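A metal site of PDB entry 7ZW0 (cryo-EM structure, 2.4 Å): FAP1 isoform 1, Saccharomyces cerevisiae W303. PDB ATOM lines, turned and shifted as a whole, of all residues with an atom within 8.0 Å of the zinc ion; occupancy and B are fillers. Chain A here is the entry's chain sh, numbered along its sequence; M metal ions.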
ATOM      1  N   LEU A 466       3.294  -2.236  -7.982  1.00  0.00           N
ATOM      2  CA  LEU A 466       2.267  -3.284  -7.946  1.00  0.00           C
ATOM      3  C   LEU A 466       1.076  -2.903  -8.812  1.00  0.00           C
ATOM      4  O   LEU A 466       1.115  -1.895  -9.522  1.00  0.00           O
ATOM      5  CB  LEU A 466       1.829  -3.560  -6.516  1.00  0.00           C
ATOM      6  CG  LEU A 466       2.900  -4.216  -5.650  1.00  0.00           C
ATOM      7  CD1 LEU A 466       2.391  -4.462  -4.236  1.00  0.00           C
ATOM      8  CD2 LEU A 466       3.351  -5.516  -6.289  1.00  0.00           C
ATOM      9  N   SER A 467       0.012  -3.702  -8.766  1.00  0.00           N
ATOM     10  CA  SER A 467      -1.155  -3.430  -9.596  1.00  0.00           C
ATOM     11  C   SER A 467      -1.723  -2.069  -9.228  1.00  0.00           C
ATOM     12  O   SER A 467      -2.139  -1.318 -10.104  1.00  0.00           O
ATOM     13  CB  SER A 467      -2.207  -4.516  -9.391  1.00  0.00           C
ATOM     14  OG  SER A 467      -2.679  -4.528  -8.058  1.00  0.00           O
ATOM     15  N   CYS A 468      -1.754  -1.747  -7.932  1.00  0.00           N
ATOM     16  CA  CYS A 468      -2.216  -0.435  -7.508  1.00  0.00           C
ATOM     17  C   CYS A 468      -1.291   0.645  -8.057  1.00  0.00           C
ATOM     18  O   CYS A 468      -1.754   1.696  -8.489  1.00  0.00           O
ATOM     19  CB  CYS A 468      -2.226  -0.367  -5.991  1.00  0.00           C
ATOM     20  SG  CYS A 468      -0.640  -0.774  -5.233  1.00  0.00           S
ATOM     21  N   GLY A 469       0.014   0.379  -8.044  1.00  0.00           N
ATOM     22  CA  GLY A 469       0.977   1.344  -8.532  1.00  0.00           C
ATOM     23  C   GLY A 469       1.448   2.299  -7.455  1.00  0.00           C
ATOM     24  O   GLY A 469       2.347   3.106  -7.686  1.00  0.00           O
ATOM     25  N   ILE A 470       0.843   2.226  -6.274  1.00  0.00           N
ATOM     26  CA  ILE A 470       1.286   3.054  -5.164  1.00  0.00           C
ATOM     27  C   ILE A 470       2.165   2.256  -4.209  1.00  0.00           C
ATOM     28  O   ILE A 470       2.599   2.783  -3.180  1.00  0.00           O
ATOM     29  CB  ILE A 470       0.102   3.688  -4.406  1.00  0.00           C
ATOM     30  CG1 ILE A 470      -0.831   2.604  -3.861  1.00  0.00           C
ATOM     31  CG2 ILE A 470      -0.665   4.630  -5.311  1.00  0.00           C
ATOM     32  CD1 ILE A 470      -2.012   3.157  -3.097  1.00  0.00           C
ATOM     33  N   HIS A 471       2.440   1.007  -4.545  1.00  0.00           N
ATOM     34  CA  HIS A 471       3.264   0.154  -3.687  1.00  0.00           C
ATOM     35  C   HIS A 471       4.363  -0.529  -4.474  1.00  0.00           C
ATOM     36  O   HIS A 471       4.248  -0.692  -5.687  1.00  0.00           O
ATOM     37  CB  HIS A 471       2.402  -0.896  -2.989  1.00  0.00           C
ATOM     38  CG  HIS A 471       1.443  -0.335  -1.979  1.00  0.00           C
ATOM     39  ND1 HIS A 471       0.076  -0.419  -2.134  1.00  0.00           N
ATOM     40  CD2 HIS A 471       1.656   0.320  -0.817  1.00  0.00           C
ATOM     41  CE1 HIS A 471      -0.514   0.163  -1.101  1.00  0.00           C
ATOM     42  NE2 HIS A 471       0.429   0.618  -0.291  1.00  0.00           N
ATOM     43  N   LYS A 472       5.426  -0.929  -3.787  1.00  0.00           N
ATOM     44  CA  LYS A 472       6.543  -1.594  -4.446  1.00  0.00           C
ATOM     45  C   LYS A 472       6.524  -3.079  -4.121  1.00  0.00           C
ATOM     46  O   LYS A 472       6.187  -3.462  -3.010  1.00  0.00           O
ATOM     47  CB  LYS A 472       7.880  -0.987  -4.018  1.00  0.00           C
ATOM     48  CG  LYS A 472       8.215   0.309  -4.736  1.00  0.00           C
ATOM     49  CD  LYS A 472       8.339   0.071  -6.226  1.00  0.00           C
ATOM     50  CE  LYS A 472       8.802   1.319  -6.969  1.00  0.00           C
ATOM     51  NZ  LYS A 472       9.005   1.052  -8.417  1.00  0.00           N
ATOM     52  N   PRO A 484      -0.761  -8.910  -7.753  1.00  0.00           N
ATOM     53  CA  PRO A 484      -1.702  -7.851  -7.367  1.00  0.00           C
ATOM     54  C   PRO A 484      -1.467  -7.408  -5.936  1.00  0.00           C
ATOM     55  O   PRO A 484      -1.099  -8.243  -5.098  1.00  0.00           O
ATOM     56  CB  PRO A 484      -3.055  -8.532  -7.500  1.00  0.00           C
ATOM     57  CG  PRO A 484      -2.847  -9.614  -8.490  1.00  0.00           C
ATOM     58  CD  PRO A 484      -1.449 -10.114  -8.246  1.00  0.00           C
ATOM     59  N   CYS A 485      -1.694  -6.135  -5.640  1.00  0.00           N
ATOM     60  CA  CYS A 485      -1.397  -5.629  -4.309  1.00  0.00           C
ATOM     61  C   CYS A 485      -2.174  -6.338  -3.215  1.00  0.00           C
ATOM     62  O   CYS A 485      -3.375  -6.573  -3.340  1.00  0.00           O
ATOM     63  CB  CYS A 485      -1.677  -4.134  -4.235  1.00  0.00           C
ATOM     64  SG  CYS A 485      -1.287  -3.383  -2.631  1.00  0.00           S
ATOM     65  N   LEU A 486      -1.486  -6.680  -2.129  1.00  0.00           N
ATOM     66  CA  LEU A 486      -2.111  -7.381  -1.018  1.00  0.00           C
ATOM     67  C   LEU A 486      -3.199  -6.560  -0.335  1.00  0.00           C
ATOM     68  O   LEU A 486      -4.234  -7.104   0.043  1.00  0.00           O
ATOM     69  CB  LEU A 486      -1.057  -7.774   0.007  1.00  0.00           C
ATOM     70  CG  LEU A 486       0.176  -8.500  -0.552  1.00  0.00           C
ATOM     71  CD1 LEU A 486       1.251  -8.637   0.508  1.00  0.00           C
ATOM     72  CD2 LEU A 486      -0.203  -9.857  -1.132  1.00  0.00           C
ATOM     73  N   GLU A 487      -2.959  -5.265  -0.183  1.00  0.00           N
ATOM     74  CA  GLU A 487      -3.916  -4.428   0.545  1.00  0.00           C
ATOM     75  C   GLU A 487      -5.282  -4.381  -0.127  1.00  0.00           C
ATOM     76  O   GLU A 487      -5.372  -4.267  -1.353  1.00  0.00           O
ATOM     77  CB  GLU A 487      -3.367  -3.013   0.690  1.00  0.00           C
ATOM     78  CG  GLU A 487      -1.933  -2.960   1.198  1.00  0.00           C
ATOM     79  CD  GLU A 487      -1.791  -3.482   2.621  1.00  0.00           C
ATOM     80  OE1 GLU A 487      -0.757  -4.117   2.915  1.00  0.00           O
ATOM     81  OE2 GLU A 487      -2.712  -3.262   3.440  1.00  0.00           O
ATOM     82  N   SER A 488      -6.340  -4.478   0.669  1.00  0.00           N
ATOM     83  CA  SER A 488      -7.683  -4.386   0.113  1.00  0.00           C
ATOM     84  C   SER A 488      -8.513  -3.343   0.851  1.00  0.00           C
ATOM     85  O   SER A 488      -8.568  -3.358   2.082  1.00  0.00           O
ATOM     86  CB  SER A 488      -8.379  -5.752   0.157  1.00  0.00           C
ATOM     87  OG  SER A 488      -8.476  -6.231   1.493  1.00  0.00           O
ATOM     88  N   ARG A 507      -9.823  -4.589  -4.163  1.00  0.00           N
ATOM     89  CA  ARG A 507      -8.376  -4.663  -4.308  1.00  0.00           C
ATOM     90  C   ARG A 507      -7.807  -3.275  -4.482  1.00  0.00           C
ATOM     91  O   ARG A 507      -8.434  -2.407  -5.078  1.00  0.00           O
ATOM     92  CB  ARG A 507      -7.995  -5.527  -5.513  1.00  0.00           C
ATOM     93  CG  ARG A 507      -7.953  -7.017  -5.223  1.00  0.00           C
ATOM     94  CD  ARG A 507      -7.456  -7.786  -6.429  1.00  0.00           C
ATOM     95  NE  ARG A 507      -7.198  -9.193  -6.128  1.00  0.00           N
ATOM     96  CZ  ARG A 507      -6.779 -10.090  -7.015  1.00  0.00           C
ATOM     97  NH1 ARG A 507      -6.570  -9.718  -8.270  1.00  0.00           N
ATOM     98  NH2 ARG A 507      -6.572 -11.347  -6.655  1.00  0.00           N
ATOM     99  N   CYS A 508      -6.623  -3.038  -3.932  1.00  0.00           N
ATOM    100  CA  CYS A 508      -6.060  -1.693  -3.990  1.00  0.00           C
ATOM    101  C   CYS A 508      -5.827  -1.304  -5.433  1.00  0.00           C
ATOM    102  O   CYS A 508      -5.337  -2.098  -6.231  1.00  0.00           O
ATOM    103  CB  CYS A 508      -4.749  -1.634  -3.209  1.00  0.00           C
ATOM    104  SG  CYS A 508      -4.196   0.042  -2.807  1.00  0.00           S
ATOM    105  N   GLY A 509      -6.184  -0.070  -5.779  1.00  0.00           N
ATOM    106  CA  GLY A 509      -6.012   0.401  -7.147  1.00  0.00           C
ATOM    107  C   GLY A 509      -7.137   0.031  -8.097  1.00  0.00           C
ATOM    108  O   GLY A 509      -7.062   0.347  -9.288  1.00  0.00           O
ATOM    109  N   THR A 510      -8.186  -0.622  -7.594  1.00  0.00           N
ATOM    110  CA  THR A 510      -9.334  -0.937  -8.443  1.00  0.00           C
ATOM    111  C   THR A 510     -10.037   0.351  -8.833  1.00  0.00           C
ATOM    112  O   THR A 510     -10.213   1.239  -8.004  1.00  0.00           O
ATOM    113  CB  THR A 510     -10.319  -1.896  -7.746  1.00  0.00           C
ATOM    114  OG1 THR A 510      -9.663  -3.139  -7.471  1.00  0.00           O
ATOM    115  CG2 THR A 510     -11.548  -2.165  -8.608  1.00  0.00           C
HETATM  116 ZN    ZN M   1      -1.800  -1.172  -3.388  1.00  0.00          ZN
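The zinc ion is bound by the side-chain sulfur of Cys 468, a ring nitrogen (ND1) of His 471, the side-chain sulfur of Cys 485 and the side-chain sulfur of Cys 508.
Merely in contact with the zinc ion: Ile 470. Within 4 Å of the zinc ion: Cys 468, Ile 470, His 471, Cys 485 and Cys 508. Along chain A the residues within 4 Å of the zinc ion span positions 468 to 508.
The side-chain sulfur of Cys 485 sits close to the backbone NH of Glu 487 (3.5 Å). O of Glu 487 sits at hydrogen-bond distance from N of Cys 508 (3.1 Å). OG of Ser 467 is in hydrogen-bond range of N of Cys 485 (3.1 Å). O of His 471 sits at hydrogen-bond distance from N of Leu 466 (2.9 Å). SG of Cys 468 sits close to N of Ile 470, at 3.5 Å.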
